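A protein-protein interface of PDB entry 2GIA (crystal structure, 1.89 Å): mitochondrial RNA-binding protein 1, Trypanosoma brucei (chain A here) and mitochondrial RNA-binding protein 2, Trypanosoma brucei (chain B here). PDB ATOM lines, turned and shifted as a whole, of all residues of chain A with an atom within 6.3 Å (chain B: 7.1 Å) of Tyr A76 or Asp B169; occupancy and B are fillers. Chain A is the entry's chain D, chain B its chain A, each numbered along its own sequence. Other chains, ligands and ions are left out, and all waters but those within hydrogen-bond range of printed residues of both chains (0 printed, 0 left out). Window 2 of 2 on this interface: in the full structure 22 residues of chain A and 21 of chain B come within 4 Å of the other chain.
Of the printed residues of chain B, Ala A75 touches Ala B171 (3.5 Å), Leu B174 (3.6 Å) and Met B175 (3.2 Å).
His A88 touches none of the printed residues of chain B.
Asp B169 touches one residue of chain A.
Of the printed residues of chain A, Val B170 touches Tyr A76 and Val A85.
The nearest residue of chain A that does not touch Asp B169 is Val A72 (5.0 Å).
The nearest printed residue of chain B that does not touch Ala A75 is Glu B172 (5.1 Å).
OD2 of Asp B169 lies within hydrogen-bond range of OH of Tyr A76.
Hydrophobic or aromatic side chains of chain A within 4 Å of the printed part of chain B: His A71, Val A72, Ala A75, Tyr A76, Val A78 and Val A85.
Along chain A the printed residues that touch a printed residue of chain B span positions 71 to 85.
Of the 16 printed residues of chain B, 5 touch a printed residue of chain A.
Hydrophobic or aromatic side chains of chain B within 4 Å of the printed part of chain A: Val B170, Ala B171, Leu B174 and Met B175.
Among the printed residues, no Asp or Glu carboxylate lies within 4 Å of a Lys or Arg side-chain nitrogen of the other chain.
Met B175 touches His A71 (CE to CD2, 3.4 Å).
Val A72 touches Ala B171 (CG2 to CB, 3.7 Å).
Ala B171 touches Ala A75 (O to CB, 3.5 Å).
O of Ala A75 touches CD2 of Leu B174, 3.6 Å away.
Met B175 touches Ala A75.
Tyr A76 touches Val B170 (CE1 to CG1, 3.2 Å).
Tyr A76 touches Ala B171 (CD2 to CB, 3.3 Å).
CG1 of Val A78 touches CD2 of Leu B174, at 3.8 Å.
Leu B174 touches Gly A79 (CD2 to N, 3.5 Å).
Val A85 touches Val B170.
The backbone NH (N) of Ala B171 lies within hydrogen-bond range of the side-chain carboxylate (OD1) of Asp B169, at 3.0 Å.
N of Asp B169 lies within hydrogen-bond range of OE1 of Glu B172.
The side-chain hydroxyl (OG) of Ser B173 is in hydrogen-bond range of the backbone carbonyl oxygen (O) of Asp B169 (2.7 Å).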
ATOM      1  N   ARG A  70       0.157 -16.483  24.498  1.00  0.00           N
ATOM      2  CA  ARG A  70       0.863 -16.886  25.725  1.00  0.00           C
ATOM      3  C   ARG A  70       0.699 -15.781  26.764  1.00  0.00           C
ATOM      4  O   ARG A  70       0.315 -14.684  26.435  1.00  0.00           O
ATOM      5  CB  ARG A  70       2.364 -17.017  25.452  1.00  0.00           C
ATOM      6  CG  ARG A  70       2.779 -18.011  24.355  1.00  0.00           C
ATOM      7  CD  ARG A  70       4.251 -17.756  23.994  1.00  0.00           C
ATOM      8  NE  ARG A  70       4.405 -16.471  23.327  1.00  0.00           N
ATOM      9  CZ  ARG A  70       5.565 -15.843  23.161  1.00  0.00           C
ATOM     10  NH1 ARG A  70       6.682 -16.395  23.635  1.00  0.00           N
ATOM     11  NH2 ARG A  70       5.612 -14.678  22.499  1.00  0.00           N
ATOM     12  N   HIS A  71       1.042 -16.060  28.012  1.00  0.00           N
ATOM     13  CA  HIS A  71       0.933 -15.051  29.058  1.00  0.00           C
ATOM     14  C   HIS A  71       1.785 -13.816  28.702  1.00  0.00           C
ATOM     15  O   HIS A  71       1.348 -12.670  28.869  1.00  0.00           O
ATOM     16  CB  HIS A  71       1.374 -15.700  30.401  1.00  0.00           C
ATOM     17  CG  HIS A  71       1.157 -14.849  31.625  1.00  0.00           C
ATOM     18  ND1 HIS A  71       0.118 -13.944  31.753  1.00  0.00           N
ATOM     19  CD2 HIS A  71       1.757 -14.896  32.844  1.00  0.00           C
ATOM     20  CE1 HIS A  71       0.082 -13.483  32.997  1.00  0.00           C
ATOM     21  NE2 HIS A  71       1.064 -14.051  33.679  1.00  0.00           N
ATOM     22  N   VAL A  72       2.986 -14.033  28.165  1.00  0.00           N
ATOM     23  CA  VAL A  72       3.853 -12.895  27.875  1.00  0.00           C
ATOM     24  C   VAL A  72       3.269 -12.037  26.735  1.00  0.00           C
ATOM     25  O   VAL A  72       3.449 -10.831  26.707  1.00  0.00           O
ATOM     26  CB  VAL A  72       5.336 -13.396  27.573  1.00  0.00           C
ATOM     27  CG1 VAL A  72       5.440 -13.993  26.172  1.00  0.00           C
ATOM     28  CG2 VAL A  72       6.311 -12.262  27.799  1.00  0.00           C
ATOM     29  N   ASP A  73       2.521 -12.665  25.831  1.00  0.00           N
ATOM     30  CA  ASP A  73       1.878 -11.919  24.733  1.00  0.00           C
ATOM     31  C   ASP A  73       0.791 -10.978  25.292  1.00  0.00           C
ATOM     32  O   ASP A  73       0.598  -9.887  24.762  1.00  0.00           O
ATOM     33  CB  ASP A  73       1.207 -12.870  23.746  1.00  0.00           C
ATOM     34  CG  ASP A  73       2.204 -13.688  22.968  1.00  0.00           C
ATOM     35  OD1 ASP A  73       3.260 -13.126  22.594  1.00  0.00           O
ATOM     36  OD2 ASP A  73       1.896 -14.865  22.718  1.00  0.00           O
ATOM     37  N   LEU A  74       0.069 -11.419  26.326  1.00  0.00           N
ATOM     38  CA  LEU A  74      -0.937 -10.558  26.948  1.00  0.00           C
ATOM     39  C   LEU A  74      -0.188  -9.305  27.496  1.00  0.00           C
ATOM     40  O   LEU A  74      -0.630  -8.144  27.306  1.00  0.00           O
ATOM     41  CB  LEU A  74      -1.667 -11.320  28.085  1.00  0.00           C
ATOM     42  CG  LEU A  74      -2.558 -10.520  29.053  1.00  0.00           C
ATOM     43  CD1 LEU A  74      -3.663  -9.735  28.270  1.00  0.00           C
ATOM     44  CD2 LEU A  74      -3.219 -11.505  30.045  1.00  0.00           C
ATOM     45  N   ALA A  75       0.956  -9.527  28.156  1.00  0.00           N
ATOM     46  CA  ALA A  75       1.728  -8.388  28.685  1.00  0.00           C
ATOM     47  C   ALA A  75       2.261  -7.480  27.551  1.00  0.00           C
ATOM     48  O   ALA A  75       2.259  -6.255  27.685  1.00  0.00           O
ATOM     49  CB  ALA A  75       2.896  -8.891  29.607  1.00  0.00           C
ATOM     50  N   TYR A  76       2.716  -8.064  26.438  1.00  0.00           N
ATOM     51  CA  TYR A  76       3.153  -7.238  25.287  1.00  0.00           C
ATOM     52  C   TYR A  76       1.961  -6.419  24.738  1.00  0.00           C
ATOM     53  O   TYR A  76       2.132  -5.242  24.388  1.00  0.00           O
ATOM     54  CB  TYR A  76       3.693  -8.116  24.144  1.00  0.00           C
ATOM     55  CG  TYR A  76       5.198  -8.237  24.133  1.00  0.00           C
ATOM     56  CD1 TYR A  76       5.972  -7.151  23.822  1.00  0.00           C
ATOM     57  CD2 TYR A  76       5.836  -9.417  24.522  1.00  0.00           C
ATOM     58  CE1 TYR A  76       7.351  -7.209  23.896  1.00  0.00           C
ATOM     59  CE2 TYR A  76       7.223  -9.478  24.596  1.00  0.00           C
ATOM     60  CZ  TYR A  76       7.960  -8.352  24.272  1.00  0.00           C
ATOM     61  OH  TYR A  76       9.335  -8.373  24.269  1.00  0.00           O
ATOM     62  N   LEU A  77       0.766  -7.024  24.666  1.00  0.00           N
ATOM     63  CA  LEU A  77      -0.400  -6.283  24.123  1.00  0.00           C
ATOM     64  C   LEU A  77      -0.700  -5.098  25.015  1.00  0.00           C
ATOM     65  O   LEU A  77      -1.008  -4.002  24.534  1.00  0.00           O
ATOM     66  CB  LEU A  77      -1.638  -7.169  24.003  1.00  0.00           C
ATOM     67  CG  LEU A  77      -1.554  -8.312  22.978  1.00  0.00           C
ATOM     68  CD1 LEU A  77      -2.956  -8.813  22.654  1.00  0.00           C
ATOM     69  CD2 LEU A  77      -0.850  -7.853  21.745  1.00  0.00           C
ATOM     70  N   VAL A  78      -0.670  -5.309  26.332  1.00  0.00           N
ATOM     71  CA  VAL A  78      -0.871  -4.182  27.220  1.00  0.00           C
ATOM     72  C   VAL A  78       0.260  -3.154  26.967  1.00  0.00           C
ATOM     73  O   VAL A  78       0.019  -1.948  26.975  1.00  0.00           O
ATOM     74  CB  VAL A  78      -0.868  -4.664  28.705  1.00  0.00           C
ATOM     75  CG1 VAL A  78      -0.835  -3.474  29.683  1.00  0.00           C
ATOM     76  CG2 VAL A  78      -2.146  -5.503  28.934  1.00  0.00           C
ATOM     77  N   GLY A  79       1.504  -3.612  26.813  1.00  0.00           N
ATOM     78  CA  GLY A  79       2.570  -2.645  26.535  1.00  0.00           C
ATOM     79  C   GLY A  79       2.317  -1.787  25.268  1.00  0.00           C
ATOM     80  O   GLY A  79       2.687  -0.598  25.203  1.00  0.00           O
ATOM     81  N   VAL A  80       1.715  -2.380  24.246  1.00  0.00           N
ATOM     82  CA  VAL A  80       1.389  -1.631  23.022  1.00  0.00           C
ATOM     83  C   VAL A  80       0.293  -0.641  23.388  1.00  0.00           C
ATOM     84  O   VAL A  80       0.336   0.517  22.958  1.00  0.00           O
ATOM     85  CB  VAL A  80       0.853  -2.547  21.905  1.00  0.00           C
ATOM     86  CG1 VAL A  80       0.271  -1.690  20.750  1.00  0.00           C
ATOM     87  CG2 VAL A  80       1.977  -3.453  21.397  1.00  0.00           C
ATOM     88  N   CYS A  81      -0.693  -1.063  24.187  1.00  0.00           N
ATOM     89  CA  CYS A  81      -1.741  -0.102  24.581  1.00  0.00           C
ATOM     90  C   CYS A  81      -1.149   1.101  25.343  1.00  0.00           C
ATOM     91  O   CYS A  81      -1.590   2.252  25.162  1.00  0.00           O
ATOM     92  CB  CYS A  81      -2.784  -0.744  25.498  1.00  0.00           C
ATOM     93  SG  CYS A  81      -3.758  -1.970  24.651  1.00  0.00           S
ATOM     94  N   VAL A  85       5.841  -0.002  23.663  1.00  0.00           N
ATOM     95  CA  VAL A  85       6.383  -0.599  22.444  1.00  0.00           C
ATOM     96  C   VAL A  85       5.394  -0.262  21.351  1.00  0.00           C
ATOM     97  O   VAL A  85       4.179  -0.239  21.591  1.00  0.00           O
ATOM     98  CB  VAL A  85       6.545  -2.151  22.479  1.00  0.00           C
ATOM     99  CG1 VAL A  85       7.728  -2.515  23.344  1.00  0.00           C
ATOM    100  CG2 VAL A  85       5.274  -2.832  22.958  1.00  0.00           C
ATOM    101  N   ARG A  87       4.732  -2.018  18.614  1.00  0.00           N
ATOM    102  CA  ARG A  87       3.983  -3.173  18.165  1.00  0.00           C
ATOM    103  C   ARG A  87       4.551  -4.472  18.682  1.00  0.00           C
ATOM    104  O   ARG A  87       5.626  -4.515  19.286  1.00  0.00           O
ATOM    105  CB  ARG A  87       3.942  -3.212  16.632  1.00  0.00           C
ATOM    106  CG  ARG A  87       5.237  -3.589  15.957  1.00  0.00           C
ATOM    107  CD  ARG A  87       4.946  -4.076  14.523  1.00  0.00           C
ATOM    108  NE  ARG A  87       6.149  -4.165  13.695  1.00  0.00           N
ATOM    109  CZ  ARG A  87       6.640  -5.289  13.170  1.00  0.00           C
ATOM    110  NH1 ARG A  87       6.040  -6.454  13.381  1.00  0.00           N
ATOM    111  NH2 ARG A  87       7.735  -5.241  12.419  1.00  0.00           N
ATOM    112  N   HIS A  88       3.808  -5.536  18.456  1.00  0.00           N
ATOM    113  CA  HIS A  88       4.239  -6.846  18.903  1.00  0.00           C
ATOM    114  C   HIS A  88       3.884  -7.837  17.835  1.00  0.00           C
ATOM    115  O   HIS A  88       2.751  -7.844  17.323  1.00  0.00           O
ATOM    116  CB  HIS A  88       3.551  -7.235  20.228  1.00  0.00           C
ATOM    117  CG  HIS A  88       3.911  -8.612  20.723  1.00  0.00           C
ATOM    118  ND1 HIS A  88       5.217  -9.020  20.898  1.00  0.00           N
ATOM    119  CD2 HIS A  88       3.137  -9.641  21.144  1.00  0.00           C
ATOM    120  CE1 HIS A  88       5.230 -10.234  21.416  1.00  0.00           C
ATOM    121  NE2 HIS A  88       3.984 -10.634  21.577  1.00  0.00           N
ATOM    122  N   PHE A  99       0.341  -6.836  16.188  1.00  0.00           N
ATOM    123  CA  PHE A  99      -0.632  -6.039  16.939  1.00  0.00           C
ATOM    124  C   PHE A  99      -0.001  -4.652  17.102  1.00  0.00           C
ATOM    125  O   PHE A  99       1.111  -4.516  17.634  1.00  0.00           O
ATOM    126  CB  PHE A  99      -0.949  -6.670  18.317  1.00  0.00           C
ATOM    127  CG  PHE A  99      -1.941  -5.851  19.139  1.00  0.00           C
ATOM    128  CD1 PHE A  99      -1.497  -4.976  20.117  1.00  0.00           C
ATOM    129  CD2 PHE A  99      -3.318  -5.978  18.936  1.00  0.00           C
ATOM    130  CE1 PHE A  99      -2.406  -4.244  20.894  1.00  0.00           C
ATOM    131  CE2 PHE A  99      -4.237  -5.254  19.695  1.00  0.00           C
ATOM    132  CZ  PHE A  99      -3.779  -4.379  20.687  1.00  0.00           C
ATOM    133  N   VAL B  48       9.296 -16.110  34.106  1.00  0.00           N
ATOM    134  CA  VAL B  48      10.144 -15.380  33.172  1.00  0.00           C
ATOM    135  C   VAL B  48      10.906 -16.557  32.570  1.00  0.00           C
ATOM    136  O   VAL B  48      11.762 -17.158  33.233  1.00  0.00           O
ATOM    137  CB  VAL B  48      11.094 -14.388  33.880  1.00  0.00           C
ATOM    138  CG1 VAL B  48      12.034 -13.707  32.846  1.00  0.00           C
ATOM    139  CG2 VAL B  48      10.234 -13.311  34.611  1.00  0.00           C
ATOM    140  N   HIS B  50      13.360 -18.222  29.818  1.00  0.00           N
ATOM    141  CA  HIS B  50      14.521 -17.979  28.949  1.00  0.00           C
ATOM    142  C   HIS B  50      15.257 -19.303  28.586  1.00  0.00           C
ATOM    143  O   HIS B  50      16.446 -19.470  28.879  1.00  0.00           O
ATOM    144  CB  HIS B  50      15.485 -17.012  29.670  1.00  0.00           C
ATOM    145  CG  HIS B  50      14.897 -15.637  29.916  1.00  0.00           C
ATOM    146  ND1 HIS B  50      15.515 -14.685  30.708  1.00  0.00           N
ATOM    147  CD2 HIS B  50      13.791 -15.040  29.400  1.00  0.00           C
ATOM    148  CE1 HIS B  50      14.823 -13.549  30.660  1.00  0.00           C
ATOM    149  NE2 HIS B  50      13.774 -13.740  29.866  1.00  0.00           N
ATOM    150  N   ALA B 133      17.282  -0.457  26.457  1.00  0.00           N
ATOM    151  CA  ALA B 133      15.926  -0.458  25.920  1.00  0.00           C
ATOM    152  C   ALA B 133      14.991   0.175  26.942  1.00  0.00           C
ATOM    153  O   ALA B 133      15.037  -0.159  28.121  1.00  0.00           O
ATOM    154  CB  ALA B 133      15.445  -1.886  25.605  1.00  0.00           C
ATOM    155  N   PRO B 134      14.137   1.096  26.494  1.00  0.00           N
ATOM    156  CA  PRO B 134      13.235   1.701  27.471  1.00  0.00           C
ATOM    157  C   PRO B 134      12.277   0.674  28.078  1.00  0.00           C
ATOM    158  O   PRO B 134      11.795  -0.300  27.429  1.00  0.00           O
ATOM    159  CB  PRO B 134      12.520   2.786  26.637  1.00  0.00           C
ATOM    160  CG  PRO B 134      12.382   2.123  25.283  1.00  0.00           C
ATOM    161  CD  PRO B 134      13.802   1.508  25.104  1.00  0.00           C
ATOM    162  N   TYR B 135      11.939   0.925  29.330  1.00  0.00           N
ATOM    163  CA  TYR B 135      11.021   0.095  30.096  1.00  0.00           C
ATOM    164  C   TYR B 135      11.484  -1.361  30.272  1.00  0.00           C
ATOM    165  O   TYR B 135      10.651  -2.270  30.378  1.00  0.00           O
ATOM    166  CB  TYR B 135       9.601   0.131  29.496  1.00  0.00           C
ATOM    167  CG  TYR B 135       9.088   1.531  29.305  1.00  0.00           C
ATOM    168  CD1 TYR B 135       9.069   2.120  28.036  1.00  0.00           C
ATOM    169  CD2 TYR B 135       8.635   2.281  30.394  1.00  0.00           C
ATOM    170  CE1 TYR B 135       8.611   3.432  27.858  1.00  0.00           C
ATOM    171  CE2 TYR B 135       8.175   3.594  30.225  1.00  0.00           C
ATOM    172  CZ  TYR B 135       8.166   4.161  28.957  1.00  0.00           C
ATOM    173  OH  TYR B 135       7.705   5.458  28.777  1.00  0.00           O
ATOM    174  N   THR B 136      12.805  -1.581  30.321  1.00  0.00           N
ATOM    175  CA  THR B 136      13.311  -2.930  30.544  1.00  0.00           C
ATOM    176  C   THR B 136      14.253  -2.776  31.737  1.00  0.00           C
ATOM    177  O   THR B 136      14.779  -1.677  32.006  1.00  0.00           O
ATOM    178  CB  THR B 136      14.098  -3.514  29.327  1.00  0.00           C
ATOM    179  OG1 THR B 136      15.271  -2.716  29.056  1.00  0.00           O
ATOM    180  CG2 THR B 136      13.177  -3.536  28.088  1.00  0.00           C
ATOM    181  N   PHE B 137      14.492  -3.900  32.410  1.00  0.00           N
ATOM    182  CA  PHE B 137      15.266  -3.893  33.665  1.00  0.00           C
ATOM    183  C   PHE B 137      16.108  -5.124  33.824  1.00  0.00           C
ATOM    184  O   PHE B 137      15.857  -6.174  33.180  1.00  0.00           O
ATOM    185  CB  PHE B 137      14.252  -3.808  34.828  1.00  0.00           C
ATOM    186  CG  PHE B 137      13.396  -2.577  34.779  1.00  0.00           C
ATOM    187  CD1 PHE B 137      13.766  -1.454  35.493  1.00  0.00           C
ATOM    188  CD2 PHE B 137      12.259  -2.516  33.956  1.00  0.00           C
ATOM    189  CE1 PHE B 137      13.014  -0.247  35.395  1.00  0.00           C
ATOM    190  CE2 PHE B 137      11.486  -1.306  33.844  1.00  0.00           C
ATOM    191  CZ  PHE B 137      11.872  -0.178  34.563  1.00  0.00           C
ATOM    192  N   GLU B 167      17.289 -10.835  32.797  1.00  0.00           N
ATOM    193  CA  GLU B 167      16.887  -9.624  32.093  1.00  0.00           C
ATOM    194  C   GLU B 167      15.348  -9.619  31.979  1.00  0.00           C
ATOM    195  O   GLU B 167      14.725 -10.647  31.728  1.00  0.00           O
ATOM    196  CB  GLU B 167      17.498  -9.590  30.677  1.00  0.00           C
ATOM    197  CG  GLU B 167      19.002  -9.516  30.644  1.00  0.00           C
ATOM    198  CD  GLU B 167      19.563  -8.230  31.190  1.00  0.00           C
ATOM    199  OE1 GLU B 167      18.779  -7.285  31.436  1.00  0.00           O
ATOM    200  OE2 GLU B 167      20.798  -8.142  31.389  1.00  0.00           O
ATOM    201  N   PHE B 168      14.723  -8.465  32.191  1.00  0.00           N
ATOM    202  CA  PHE B 168      13.251  -8.396  32.070  1.00  0.00           C
ATOM    203  C   PHE B 168      13.021  -7.487  30.877  1.00  0.00           C
ATOM    204  O   PHE B 168      13.396  -6.305  30.960  1.00  0.00           O
ATOM    205  CB  PHE B 168      12.631  -7.730  33.318  1.00  0.00           C
ATOM    206  CG  PHE B 168      12.589  -8.634  34.519  1.00  0.00           C
ATOM    207  CD1 PHE B 168      11.391  -9.184  34.933  1.00  0.00           C
ATOM    208  CD2 PHE B 168      13.755  -8.906  35.233  1.00  0.00           C
ATOM    209  CE1 PHE B 168      11.320 -10.020  36.088  1.00  0.00           C
ATOM    210  CE2 PHE B 168      13.731  -9.727  36.373  1.00  0.00           C
ATOM    211  CZ  PHE B 168      12.516 -10.288  36.810  1.00  0.00           C
ATOM    212  N   ASP B 169      12.418  -8.014  29.805  1.00  0.00           N
ATOM    213  CA  ASP B 169      12.159  -7.184  28.622  1.00  0.00           C
ATOM    214  C   ASP B 169      10.915  -6.333  28.890  1.00  0.00           C
ATOM    215  O   ASP B 169      10.431  -6.296  30.031  1.00  0.00           O
ATOM    216  CB  ASP B 169      12.031  -8.051  27.332  1.00  0.00           C
ATOM    217  CG  ASP B 169      10.794  -8.952  27.310  1.00  0.00           C
ATOM    218  OD1 ASP B 169       9.874  -8.751  28.113  1.00  0.00           O
ATOM    219  OD2 ASP B 169      10.732  -9.880  26.463  1.00  0.00           O
ATOM    220  N   VAL B 170      10.391  -5.639  27.885  1.00  0.00           N
ATOM    221  CA  VAL B 170       9.246  -4.754  28.155  1.00  0.00           C
ATOM    222  C   VAL B 170       8.035  -5.486  28.712  1.00  0.00           C
ATOM    223  O   VAL B 170       7.370  -4.976  29.613  1.00  0.00           O
ATOM    224  CB  VAL B 170       8.842  -3.951  26.877  1.00  0.00           C
ATOM    225  CG1 VAL B 170       8.417  -4.909  25.789  1.00  0.00           C
ATOM    226  CG2 VAL B 170       7.693  -3.005  27.182  1.00  0.00           C
ATOM    227  N   ALA B 171       7.741  -6.672  28.186  1.00  0.00           N
ATOM    228  CA  ALA B 171       6.596  -7.428  28.679  1.00  0.00           C
ATOM    229  C   ALA B 171       6.821  -7.997  30.086  1.00  0.00           C
ATOM    230  O   ALA B 171       5.941  -7.915  30.935  1.00  0.00           O
ATOM    231  CB  ALA B 171       6.250  -8.568  27.712  1.00  0.00           C
ATOM    232  N   GLU B 172       7.985  -8.596  30.307  1.00  0.00           N
ATOM    233  CA  GLU B 172       8.315  -9.183  31.606  1.00  0.00           C
ATOM    234  C   GLU B 172       8.364  -8.087  32.674  1.00  0.00           C
ATOM    235  O   GLU B 172       7.990  -8.323  33.824  1.00  0.00           O
ATOM    236  CB  GLU B 172       9.690  -9.888  31.492  1.00  0.00           C
ATOM    237  CG  GLU B 172       9.590 -11.074  30.516  1.00  0.00           C
ATOM    238  CD  GLU B 172      10.927 -11.530  29.915  1.00  0.00           C
ATOM    239  OE1 GLU B 172      11.925 -10.776  29.898  1.00  0.00           O
ATOM    240  OE2 GLU B 172      10.937 -12.672  29.442  1.00  0.00           O
ATOM    241  N   SER B 173       8.867  -6.907  32.307  1.00  0.00           N
ATOM    242  CA  SER B 173       8.936  -5.813  33.250  1.00  0.00           C
ATOM    243  C   SER B 173       7.512  -5.375  33.633  1.00  0.00           C
ATOM    244  O   SER B 173       7.201  -5.108  34.818  1.00  0.00           O
ATOM    245  CB  SER B 173       9.737  -4.647  32.649  1.00  0.00           C
ATOM    246  OG  SER B 173      11.100  -5.062  32.384  1.00  0.00           O
ATOM    247  N   LEU B 174       6.644  -5.277  32.627  1.00  0.00           N
ATOM    248  CA  LEU B 174       5.260  -4.863  32.879  1.00  0.00           C
ATOM    249  C   LEU B 174       4.561  -5.930  33.732  1.00  0.00           C
ATOM    250  O   LEU B 174       3.795  -5.597  34.649  1.00  0.00           O
ATOM    251  CB  LEU B 174       4.540  -4.660  31.536  1.00  0.00           C
ATOM    252  CG  LEU B 174       3.143  -4.056  31.438  1.00  0.00           C
ATOM    253  CD1 LEU B 174       2.960  -2.876  32.407  1.00  0.00           C
ATOM    254  CD2 LEU B 174       2.982  -3.555  29.975  1.00  0.00           C
ATOM    255  N   MET B 175       4.825  -7.217  33.459  1.00  0.00           N
ATOM    256  CA  MET B 175       4.222  -8.246  34.284  1.00  0.00           C
ATOM    257  C   MET B 175       4.702  -8.123  35.723  1.00  0.00           C
ATOM    258  O   MET B 175       3.915  -8.329  36.659  1.00  0.00           O
ATOM    259  CB  MET B 175       4.588  -9.657  33.766  1.00  0.00           C
ATOM    260  CG  MET B 175       4.075  -9.922  32.357  1.00  0.00           C
ATOM    261  SD  MET B 175       4.706 -11.552  31.757  1.00  0.00           S
ATOM    262  CE  MET B 175       4.099 -12.444  33.087  1.00  0.00           C
